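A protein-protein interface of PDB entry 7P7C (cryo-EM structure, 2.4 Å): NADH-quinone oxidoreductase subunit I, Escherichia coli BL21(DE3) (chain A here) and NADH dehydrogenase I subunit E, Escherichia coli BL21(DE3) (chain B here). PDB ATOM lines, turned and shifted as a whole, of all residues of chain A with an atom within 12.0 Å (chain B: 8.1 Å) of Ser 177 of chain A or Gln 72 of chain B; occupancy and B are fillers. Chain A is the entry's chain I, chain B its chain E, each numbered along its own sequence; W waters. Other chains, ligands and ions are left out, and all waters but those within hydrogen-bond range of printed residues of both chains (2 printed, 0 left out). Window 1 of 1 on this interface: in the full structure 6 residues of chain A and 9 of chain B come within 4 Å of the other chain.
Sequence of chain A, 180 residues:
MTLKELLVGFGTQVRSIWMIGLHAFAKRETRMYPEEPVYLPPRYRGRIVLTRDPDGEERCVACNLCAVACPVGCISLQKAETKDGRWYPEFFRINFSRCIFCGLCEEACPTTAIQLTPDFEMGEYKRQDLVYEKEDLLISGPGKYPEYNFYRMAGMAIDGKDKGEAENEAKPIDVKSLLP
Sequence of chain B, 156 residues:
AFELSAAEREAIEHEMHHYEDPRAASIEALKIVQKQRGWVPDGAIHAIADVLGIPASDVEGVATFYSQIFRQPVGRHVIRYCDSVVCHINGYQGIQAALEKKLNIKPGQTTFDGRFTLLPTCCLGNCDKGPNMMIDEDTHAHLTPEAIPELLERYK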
ATOM      1  N   LYS A 171      -0.396 -25.989  -6.261  1.00  0.00           N
ATOM      2  CA  LYS A 171       0.267 -24.810  -6.791  1.00  0.00           C
ATOM      3  C   LYS A 171       1.653 -25.186  -7.310  1.00  0.00           C
ATOM      4  O   LYS A 171       2.295 -26.085  -6.761  1.00  0.00           O
ATOM      5  CB  LYS A 171       0.381 -23.727  -5.715  1.00  0.00           C
ATOM      6  CG  LYS A 171      -0.926 -23.011  -5.317  1.00  0.00           C
ATOM      7  CD  LYS A 171      -1.252 -21.745  -6.138  1.00  0.00           C
ATOM      8  CE  LYS A 171      -1.731 -21.999  -7.569  1.00  0.00           C
ATOM      9  NZ  LYS A 171      -2.187 -20.759  -8.253  1.00  0.00           N
ATOM     10  N   PRO A 172       2.121 -24.549  -8.384  1.00  0.00           N
ATOM     11  CA  PRO A 172       3.449 -24.883  -8.909  1.00  0.00           C
ATOM     12  C   PRO A 172       4.552 -24.497  -7.938  1.00  0.00           C
ATOM     13  O   PRO A 172       4.515 -23.439  -7.308  1.00  0.00           O
ATOM     14  CB  PRO A 172       3.536 -24.072 -10.208  1.00  0.00           C
ATOM     15  CG  PRO A 172       2.519 -23.000 -10.065  1.00  0.00           C
ATOM     16  CD  PRO A 172       1.421 -23.571  -9.232  1.00  0.00           C
ATOM     17  N   ILE A 173       5.534 -25.380  -7.816  1.00  0.00           N
ATOM     18  CA  ILE A 173       6.709 -25.157  -6.986  1.00  0.00           C
ATOM     19  C   ILE A 173       7.869 -24.886  -7.928  1.00  0.00           C
ATOM     20  O   ILE A 173       8.257 -25.755  -8.717  1.00  0.00           O
ATOM     21  CB  ILE A 173       7.002 -26.350  -6.069  1.00  0.00           C
ATOM     22  CG1 ILE A 173       5.768 -26.699  -5.236  1.00  0.00           C
ATOM     23  CG2 ILE A 173       8.186 -26.045  -5.171  1.00  0.00           C
ATOM     24  CD1 ILE A 173       5.892 -28.001  -4.483  1.00  0.00           C
ATOM     25  N   ASP A 174       8.414 -23.680  -7.858  1.00  0.00           N
ATOM     26  CA  ASP A 174       9.522 -23.310  -8.720  1.00  0.00           C
ATOM     27  C   ASP A 174      10.795 -24.007  -8.246  1.00  0.00           C
ATOM     28  O   ASP A 174      10.967 -24.288  -7.059  1.00  0.00           O
ATOM     29  CB  ASP A 174       9.682 -21.790  -8.726  1.00  0.00           C
ATOM     30  CG  ASP A 174      10.816 -21.322  -9.601  1.00  0.00           C
ATOM     31  OD1 ASP A 174      10.622 -21.220 -10.828  1.00  0.00           O
ATOM     32  OD2 ASP A 174      11.898 -21.048  -9.061  1.00  0.00           O
ATOM     33  N   VAL A 175      11.687 -24.307  -9.195  1.00  0.00           N
ATOM     34  CA  VAL A 175      12.886 -25.079  -8.878  1.00  0.00           C
ATOM     35  C   VAL A 175      13.886 -24.290  -8.044  1.00  0.00           C
ATOM     36  O   VAL A 175      14.789 -24.885  -7.448  1.00  0.00           O
ATOM     37  CB  VAL A 175      13.564 -25.593 -10.162  1.00  0.00           C
ATOM     38  CG1 VAL A 175      12.742 -26.701 -10.783  1.00  0.00           C
ATOM     39  CG2 VAL A 175      13.777 -24.455 -11.147  1.00  0.00           C
ATOM     40  N   LYS A 176      13.752 -22.971  -7.974  1.00  0.00           N
ATOM     41  CA  LYS A 176      14.624 -22.149  -7.151  1.00  0.00           C
ATOM     42  C   LYS A 176      14.108 -21.979  -5.729  1.00  0.00           C
ATOM     43  O   LYS A 176      14.652 -21.158  -4.984  1.00  0.00           O
ATOM     44  CB  LYS A 176      14.827 -20.778  -7.796  1.00  0.00           C
ATOM     45  CG  LYS A 176      15.160 -20.830  -9.273  1.00  0.00           C
ATOM     46  CD  LYS A 176      15.191 -19.440  -9.874  1.00  0.00           C
ATOM     47  CE  LYS A 176      15.319 -19.494 -11.385  1.00  0.00           C
ATOM     48  NZ  LYS A 176      14.181 -20.219 -12.020  1.00  0.00           N
ATOM     49  N   SER A 177      13.076 -22.724  -5.341  1.00  0.00           N
ATOM     50  CA  SER A 177      12.521 -22.613  -4.000  1.00  0.00           C
ATOM     51  C   SER A 177      13.501 -23.141  -2.959  1.00  0.00           C
ATOM     52  O   SER A 177      14.271 -24.070  -3.211  1.00  0.00           O
ATOM     53  CB  SER A 177      11.199 -23.373  -3.899  1.00  0.00           C
ATOM     54  OG  SER A 177      11.409 -24.706  -3.468  1.00  0.00           O
ATOM     55  N   LEU A 178      13.462 -22.531  -1.775  1.00  0.00           N
ATOM     56  CA  LEU A 178      14.404 -22.856  -0.714  1.00  0.00           C
ATOM     57  C   LEU A 178      14.079 -24.161  -0.004  1.00  0.00           C
ATOM     58  O   LEU A 178      14.961 -24.728   0.648  1.00  0.00           O
ATOM     59  CB  LEU A 178      14.447 -21.723   0.307  1.00  0.00           C
ATOM     60  CG  LEU A 178      14.745 -20.341  -0.264  1.00  0.00           C
ATOM     61  CD1 LEU A 178      14.410 -19.266   0.750  1.00  0.00           C
ATOM     62  CD2 LEU A 178      16.198 -20.254  -0.692  1.00  0.00           C
ATOM     63  N   LEU A 179      12.847 -24.641  -0.108  1.00  0.00           N
ATOM     64  CA  LEU A 179      12.468 -25.862   0.582  1.00  0.00           C
ATOM     65  C   LEU A 179      13.103 -27.073  -0.098  1.00  0.00           C
ATOM     66  O   LEU A 179      13.222 -27.104  -1.325  1.00  0.00           O
ATOM     67  CB  LEU A 179      10.947 -26.006   0.607  1.00  0.00           C
ATOM     68  CG  LEU A 179      10.223 -25.035   1.538  1.00  0.00           C
ATOM     69  CD1 LEU A 179       8.725 -25.070   1.294  1.00  0.00           C
ATOM     70  CD2 LEU A 179      10.541 -25.355   2.987  1.00  0.00           C
ATOM     71  N   PRO A 180      13.530 -28.086   0.674  1.00  0.00           N
ATOM     72  CA  PRO A 180      14.143 -29.296   0.113  1.00  0.00           C
ATOM     73  C   PRO A 180      13.163 -30.131  -0.711  1.00  0.00           C
ATOM     74  O   PRO A 180      11.953 -29.999  -0.528  1.00  0.00           O
ATOM     75  CB  PRO A 180      14.598 -30.071   1.353  1.00  0.00           C
ATOM     76  CG  PRO A 180      14.614 -29.075   2.460  1.00  0.00           C
ATOM     77  CD  PRO A 180      13.536 -28.101   2.145  1.00  0.00           C
ATOM     78  N   GLN B  34      27.693 -17.952  -2.975  1.00  0.00           N
ATOM     79  CA  GLN B  34      26.690 -17.939  -1.916  1.00  0.00           C
ATOM     80  C   GLN B  34      27.267 -17.433  -0.598  1.00  0.00           C
ATOM     81  O   GLN B  34      26.609 -16.674   0.120  1.00  0.00           O
ATOM     82  CB  GLN B  34      26.104 -19.340  -1.746  1.00  0.00           C
ATOM     83  CG  GLN B  34      25.189 -19.504  -0.551  1.00  0.00           C
ATOM     84  CD  GLN B  34      24.149 -20.574  -0.766  1.00  0.00           C
ATOM     85  OE1 GLN B  34      23.472 -20.598  -1.789  1.00  0.00           O
ATOM     86  NE2 GLN B  34      24.017 -21.472   0.200  1.00  0.00           N
ATOM     87  N   GLY B  38      25.309 -14.322   0.273  1.00  0.00           N
ATOM     88  CA  GLY B  38      24.156 -14.863   0.962  1.00  0.00           C
ATOM     89  C   GLY B  38      23.377 -15.883   0.155  1.00  0.00           C
ATOM     90  O   GLY B  38      22.798 -16.807   0.731  1.00  0.00           O
ATOM     91  N   TRP B  39      23.361 -15.737  -1.165  1.00  0.00           N
ATOM     92  CA  TRP B  39      22.668 -16.648  -2.064  1.00  0.00           C
ATOM     93  C   TRP B  39      23.295 -16.491  -3.444  1.00  0.00           C
ATOM     94  O   TRP B  39      24.217 -15.696  -3.636  1.00  0.00           O
ATOM     95  CB  TRP B  39      21.157 -16.379  -2.084  1.00  0.00           C
ATOM     96  CG  TRP B  39      20.768 -15.044  -2.645  1.00  0.00           C
ATOM     97  CD1 TRP B  39      21.108 -13.816  -2.160  1.00  0.00           C
ATOM     98  CD2 TRP B  39      19.954 -14.806  -3.798  1.00  0.00           C
ATOM     99  NE1 TRP B  39      20.562 -12.829  -2.940  1.00  0.00           N
ATOM    100  CE2 TRP B  39      19.848 -13.411  -3.953  1.00  0.00           C
ATOM    101  CE3 TRP B  39      19.308 -15.636  -4.718  1.00  0.00           C
ATOM    102  CZ2 TRP B  39      19.121 -12.829  -4.987  1.00  0.00           C
ATOM    103  CZ3 TRP B  39      18.587 -15.057  -5.741  1.00  0.00           C
ATOM    104  CH2 TRP B  39      18.499 -13.667  -5.868  1.00  0.00           C
ATOM    105  N   VAL B  40      22.793 -17.258  -4.404  1.00  0.00           N
ATOM    106  CA  VAL B  40      23.297 -17.223  -5.771  1.00  0.00           C
ATOM    107  C   VAL B  40      22.258 -16.509  -6.634  1.00  0.00           C
ATOM    108  O   VAL B  40      21.198 -17.082  -6.925  1.00  0.00           O
ATOM    109  CB  VAL B  40      23.591 -18.630  -6.306  1.00  0.00           C
ATOM    110  CG1 VAL B  40      24.093 -18.556  -7.736  1.00  0.00           C
ATOM    111  CG2 VAL B  40      24.604 -19.336  -5.417  1.00  0.00           C
ATOM    112  N   PRO B  41      22.510 -15.279  -7.065  1.00  0.00           N
ATOM    113  CA  PRO B  41      21.560 -14.566  -7.924  1.00  0.00           C
ATOM    114  C   PRO B  41      21.630 -15.073  -9.363  1.00  0.00           C
ATOM    115  O   PRO B  41      22.417 -15.953  -9.701  1.00  0.00           O
ATOM    116  CB  PRO B  41      22.009 -13.108  -7.809  1.00  0.00           C
ATOM    117  CG  PRO B  41      23.438 -13.178  -7.449  1.00  0.00           C
ATOM    118  CD  PRO B  41      23.643 -14.431  -6.658  1.00  0.00           C
ATOM    119  N   ASP B  42      20.776 -14.491 -10.212  1.00  0.00           N
ATOM    120  CA  ASP B  42      20.579 -15.008 -11.566  1.00  0.00           C
ATOM    121  C   ASP B  42      21.812 -14.819 -12.443  1.00  0.00           C
ATOM    122  O   ASP B  42      22.167 -15.714 -13.219  1.00  0.00           O
ATOM    123  CB  ASP B  42      19.367 -14.340 -12.212  1.00  0.00           C
ATOM    124  CG  ASP B  42      18.070 -14.663 -11.500  1.00  0.00           C
ATOM    125  OD1 ASP B  42      18.067 -15.564 -10.638  1.00  0.00           O
ATOM    126  OD2 ASP B  42      17.047 -14.014 -11.806  1.00  0.00           O
ATOM    127  N   ALA B  63      22.837 -25.934  -9.459  1.00  0.00           N
ATOM    128  CA  ALA B  63      22.395 -25.037  -8.393  1.00  0.00           C
ATOM    129  C   ALA B  63      20.998 -25.386  -7.896  1.00  0.00           C
ATOM    130  O   ALA B  63      20.729 -25.319  -6.693  1.00  0.00           O
ATOM    131  CB  ALA B  63      22.442 -23.589  -8.876  1.00  0.00           C
ATOM    132  N   THR B  64      20.096 -25.762  -8.802  1.00  0.00           N
ATOM    133  CA  THR B  64      18.752 -26.140  -8.396  1.00  0.00           C
ATOM    134  C   THR B  64      18.660 -27.584  -7.926  1.00  0.00           C
ATOM    135  O   THR B  64      17.654 -27.953  -7.315  1.00  0.00           O
ATOM    136  CB  THR B  64      17.767 -25.912  -9.542  1.00  0.00           C
ATOM    137  OG1 THR B  64      18.231 -26.595 -10.710  1.00  0.00           O
ATOM    138  CG2 THR B  64      17.638 -24.432  -9.844  1.00  0.00           C
ATOM    139  N   TYR B  66      20.951 -28.998  -5.735  1.00  0.00           N
ATOM    140  CA  TYR B  66      21.447 -29.074  -4.368  1.00  0.00           C
ATOM    141  C   TYR B  66      20.698 -28.095  -3.476  1.00  0.00           C
ATOM    142  O   TYR B  66      20.556 -26.916  -3.813  1.00  0.00           O
ATOM    143  CB  TYR B  66      22.949 -28.803  -4.335  1.00  0.00           C
ATOM    144  CG  TYR B  66      23.740 -29.890  -5.019  1.00  0.00           C
ATOM    145  CD1 TYR B  66      23.976 -31.102  -4.393  1.00  0.00           C
ATOM    146  CD2 TYR B  66      24.230 -29.714  -6.302  1.00  0.00           C
ATOM    147  CE1 TYR B  66      24.684 -32.096  -5.023  1.00  0.00           C
ATOM    148  CE2 TYR B  66      24.936 -30.701  -6.939  1.00  0.00           C
ATOM    149  CZ  TYR B  66      25.162 -31.891  -6.295  1.00  0.00           C
ATOM    150  OH  TYR B  66      25.871 -32.880  -6.930  1.00  0.00           O
ATOM    151  N   SER B  67      20.225 -28.593  -2.333  1.00  0.00           N
ATOM    152  CA  SER B  67      19.331 -27.814  -1.485  1.00  0.00           C
ATOM    153  C   SER B  67      20.056 -26.692  -0.756  1.00  0.00           C
ATOM    154  O   SER B  67      19.437 -25.674  -0.427  1.00  0.00           O
ATOM    155  CB  SER B  67      18.633 -28.733  -0.484  1.00  0.00           C
ATOM    156  OG  SER B  67      19.564 -29.586   0.156  1.00  0.00           O
ATOM    157  N   GLN B  68      21.352 -26.845  -0.495  1.00  0.00           N
ATOM    158  CA  GLN B  68      22.084 -25.826   0.243  1.00  0.00           C
ATOM    159  C   GLN B  68      22.599 -24.700  -0.639  1.00  0.00           C
ATOM    160  O   GLN B  68      23.183 -23.747  -0.118  1.00  0.00           O
ATOM    161  CB  GLN B  68      23.248 -26.457   1.009  1.00  0.00           C
ATOM    162  CG  GLN B  68      22.817 -27.326   2.175  1.00  0.00           C
ATOM    163  CD  GLN B  68      21.563 -26.814   2.857  1.00  0.00           C
ATOM    164  OE1 GLN B  68      21.566 -25.744   3.465  1.00  0.00           O
ATOM    165  NE2 GLN B  68      20.484 -27.580   2.761  1.00  0.00           N
ATOM    166  N   ILE B  69      22.405 -24.782  -1.950  1.00  0.00           N
ATOM    167  CA  ILE B  69      22.706 -23.675  -2.845  1.00  0.00           C
ATOM    168  C   ILE B  69      21.411 -22.905  -3.055  1.00  0.00           C
ATOM    169  O   ILE B  69      20.485 -23.390  -3.709  1.00  0.00           O
ATOM    170  CB  ILE B  69      23.299 -24.162  -4.172  1.00  0.00           C
ATOM    171  CG1 ILE B  69      24.627 -24.874  -3.916  1.00  0.00           C
ATOM    172  CG2 ILE B  69      23.497 -22.995  -5.120  1.00  0.00           C
ATOM    173  CD1 ILE B  69      25.140 -25.655  -5.095  1.00  0.00           C
ATOM    174  N   PHE B  70      21.339 -21.706  -2.490  1.00  0.00           N
ATOM    175  CA  PHE B  70      20.107 -20.934  -2.467  1.00  0.00           C
ATOM    176  C   PHE B  70      19.998 -20.117  -3.745  1.00  0.00           C
ATOM    177  O   PHE B  70      20.900 -19.338  -4.071  1.00  0.00           O
ATOM    178  CB  PHE B  70      20.061 -20.032  -1.237  1.00  0.00           C
ATOM    179  CG  PHE B  70      20.167 -20.775   0.061  1.00  0.00           C
ATOM    180  CD1 PHE B  70      19.551 -22.006   0.223  1.00  0.00           C
ATOM    181  CD2 PHE B  70      20.885 -20.249   1.118  1.00  0.00           C
ATOM    182  CE1 PHE B  70      19.650 -22.694   1.414  1.00  0.00           C
ATOM    183  CE2 PHE B  70      20.985 -20.934   2.313  1.00  0.00           C
ATOM    184  CZ  PHE B  70      20.367 -22.156   2.460  1.00  0.00           C
ATOM    185  N   ARG B  71      18.900 -20.302  -4.470  1.00  0.00           N
ATOM    186  CA  ARG B  71      18.624 -19.557  -5.688  1.00  0.00           C
ATOM    187  C   ARG B  71      17.506 -18.543  -5.496  1.00  0.00           C
ATOM    188  O   ARG B  71      17.028 -17.962  -6.475  1.00  0.00           O
ATOM    189  CB  ARG B  71      18.294 -20.521  -6.826  1.00  0.00           C
ATOM    190  CG  ARG B  71      19.513 -21.139  -7.477  1.00  0.00           C
ATOM    191  CD  ARG B  71      20.341 -20.085  -8.170  1.00  0.00           C
ATOM    192  NE  ARG B  71      19.829 -19.813  -9.506  1.00  0.00           N
ATOM    193  CZ  ARG B  71      19.316 -18.654  -9.891  1.00  0.00           C
ATOM    194  NH1 ARG B  71      19.240 -17.623  -9.065  1.00  0.00           N
ATOM    195  NH2 ARG B  71      18.868 -18.524 -11.135  1.00  0.00           N
ATOM    196  N   GLN B  72      17.077 -18.330  -4.261  1.00  0.00           N
ATOM    197  CA  GLN B  72      16.160 -17.280  -3.855  1.00  0.00           C
ATOM    198  C   GLN B  72      16.762 -16.566  -2.656  1.00  0.00           C
ATOM    199  O   GLN B  72      17.518 -17.176  -1.895  1.00  0.00           O
ATOM    200  CB  GLN B  72      14.780 -17.852  -3.495  1.00  0.00           C
ATOM    201  CG  GLN B  72      13.836 -17.950  -4.676  1.00  0.00           C
ATOM    202  CD  GLN B  72      12.595 -18.753  -4.361  1.00  0.00           C
ATOM    203  OE1 GLN B  72      12.315 -19.052  -3.202  1.00  0.00           O
ATOM    204  NE2 GLN B  72      11.843 -19.108  -5.394  1.00  0.00           N
ATOM    205  N   PRO B  73      16.485 -15.270  -2.487  1.00  0.00           N
ATOM    206  CA  PRO B  73      17.111 -14.525  -1.386  1.00  0.00           C
ATOM    207  C   PRO B  73      16.676 -15.038  -0.022  1.00  0.00           C
ATOM    208  O   PRO B  73      15.526 -15.429   0.183  1.00  0.00           O
ATOM    209  CB  PRO B  73      16.644 -13.084  -1.622  1.00  0.00           C
ATOM    210  CG  PRO B  73      15.456 -13.199  -2.505  1.00  0.00           C
ATOM    211  CD  PRO B  73      15.707 -14.384  -3.368  1.00  0.00           C
ATOM    212  N   VAL B  74      17.621 -15.036   0.915  1.00  0.00           N
ATOM    213  CA  VAL B  74      17.392 -15.501   2.272  1.00  0.00           C
ATOM    214  C   VAL B  74      17.699 -14.360   3.232  1.00  0.00           C
ATOM    215  O   VAL B  74      18.218 -13.313   2.845  1.00  0.00           O
ATOM    216  CB  VAL B  74      18.236 -16.745   2.618  1.00  0.00           C
ATOM    217  CG1 VAL B  74      17.758 -17.947   1.830  1.00  0.00           C
ATOM    218  CG2 VAL B  74      19.708 -16.479   2.354  1.00  0.00           C
ATOM    219  N   GLY B  75      17.370 -14.578   4.501  1.00  0.00           N
ATOM    220  CA  GLY B  75      17.677 -13.616   5.533  1.00  0.00           C
ATOM    221  C   GLY B  75      19.148 -13.620   5.889  1.00  0.00           C
ATOM    222  O   GLY B  75      19.949 -14.397   5.370  1.00  0.00           O
ATOM    223  N   GLY B 108      10.451 -22.141   5.181  1.00  0.00           N
ATOM    224  CA  GLY B 108      10.688 -21.692   3.829  1.00  0.00           C
ATOM    225  C   GLY B 108      10.492 -20.210   3.609  1.00  0.00           C
ATOM    226  O   GLY B 108      10.695 -19.737   2.484  1.00  0.00           O
ATOM    227  N   THR B 110      10.981 -15.964   5.032  1.00  0.00           N
ATOM    228  CA  THR B 110      11.903 -15.045   5.677  1.00  0.00           C
ATOM    229  C   THR B 110      11.099 -14.060   6.517  1.00  0.00           C
ATOM    230  O   THR B 110       9.980 -13.686   6.156  1.00  0.00           O
ATOM    231  CB  THR B 110      12.754 -14.301   4.630  1.00  0.00           C
ATOM    232  OG1 THR B 110      13.293 -15.249   3.700  1.00  0.00           O
ATOM    233  CG2 THR B 110      13.911 -13.555   5.278  1.00  0.00           C
ATOM    234  N   THR B 117      15.696 -16.767   8.208  1.00  0.00           N
ATOM    235  CA  THR B 117      15.032 -17.630   7.240  1.00  0.00           C
ATOM    236  C   THR B 117      14.914 -19.015   7.858  1.00  0.00           C
ATOM    237  O   THR B 117      15.926 -19.621   8.223  1.00  0.00           O
ATOM    238  CB  THR B 117      15.807 -17.686   5.921  1.00  0.00           C
ATOM    239  OG1 THR B 117      15.614 -16.464   5.201  1.00  0.00           O
ATOM    240  CG2 THR B 117      15.323 -18.842   5.061  1.00  0.00           C
ATOM    241  N   LEU B 119      14.164 -22.954   7.741  1.00  0.00           N
ATOM    242  CA  LEU B 119      14.243 -24.031   6.775  1.00  0.00           C
ATOM    243  C   LEU B 119      14.311 -25.371   7.497  1.00  0.00           C
ATOM    244  O   LEU B 119      15.140 -25.541   8.412  1.00  0.00           O
ATOM    245  CB  LEU B 119      15.464 -23.867   5.865  1.00  0.00           C
ATOM    246  CG  LEU B 119      15.446 -22.753   4.819  1.00  0.00           C
ATOM    247  CD1 LEU B 119      16.760 -22.720   4.068  1.00  0.00           C
ATOM    248  CD2 LEU B 119      14.284 -22.932   3.862  1.00  0.00           C
HETATM  249  O   HOH W   1      16.819 -22.358  -3.656  1.00  0.00           O
HETATM  250  O   HOH W   2      17.489 -24.743  -2.143  1.00  0.00           O
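The side-chain amide oxygen (OE1) of Gln 34 of chain B sits at hydrogen-bond distance from the backbone NH (N) of Phe 70 of chain B (2.5 Å). NH1 of Arg 71 of chain B lies within salt-bridge range of OD1 of Asp 42 of chain B. The backbone carbonyl oxygen (O) of Phe 70 of chain B lies within hydrogen-bond range of the backbone NH (N) of Val 40 of chain B, 2.8 Å away. The side-chain carboxylate (OD2) of Asp 174 of chain A lies within salt-bridge range of the side-chain amino group (NZ) of Lys 176 of chain A (3.8 Å). The backbone carbonyl oxygen (O) of Val 40 of chain B is in hydrogen-bond range of the guanidinium group (NH1) of Arg 71 of chain B, 3.0 Å away.
Of chain A, only Lys 176, Ser 177 and Leu 178 come within 4 Å of Gln 72 of chain B. No residue of chain A comes within 4 Å of Val 40 of chain B. Phe 70 of chain B touches one residue of chain A. Arg 71 of chain B touches just one residue of chain A: Lys 176. No residue of chain A comes within 4 Å of Pro 73 of chain B. Printed residues of chain B within 4 Å of Leu 178 of chain A: Phe 70, Gln 72, Val 74 and Leu 119. Printed residues of chain B within 4 Å of Leu 179 of chain A: Gly 108 (3.8 Å). Printed residues of chain A within 4 Å of Thr 64 of chain B: Val 175. Printed residues of chain B within 4 Å of Val 175 of chain A: Thr 64. Printed residues of chain A within 4 Å of Leu 119 of chain B: Leu 178 (3.7 Å). Asp 174 of chain A touches none of the printed residues of chain B. The nearest residue of chain A that does not touch Gln 72 of chain B is Asp 174 of chain A (4.1 Å). The nearest printed residue of chain A that does not touch Leu 119 of chain B is Leu 179 of chain A (4.5 Å).
Water W2 lies within hydrogen-bond range of O of Ser 67 of chain B (2.8 Å) and O of Ser 177 of chain A (3.5 Å). Water W1 lies within hydrogen-bond range of O of Lys 176 of chain A, N of Arg 71 of chain B and O of Ser 177 of chain A.
Val 175 of chain A touches Thr 64 of chain B. Lys 176 of chain A touches Arg 71 of chain B (CB to CB, 3.6 Å). Lys 176 of chain A touches Gln 72 of chain B. CA of Ser 177 of chain A touches OE1 of Gln 72 of chain B (3.7 Å). Leu 178 of chain A touches Phe 70 of chain B (CD2 to CD1, 3.9 Å). CD2 of Leu 178 of chain A touches O of Gln 72 of chain B, at 3.6 Å. Val 74 of chain B touches Leu 178 of chain A. Leu 178 of chain A touches Leu 119 of chain B (O to CD2, 3.7 Å). Leu 179 of chain A touches Gly 108 of chain B (CD2 to CA, 3.8 Å).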
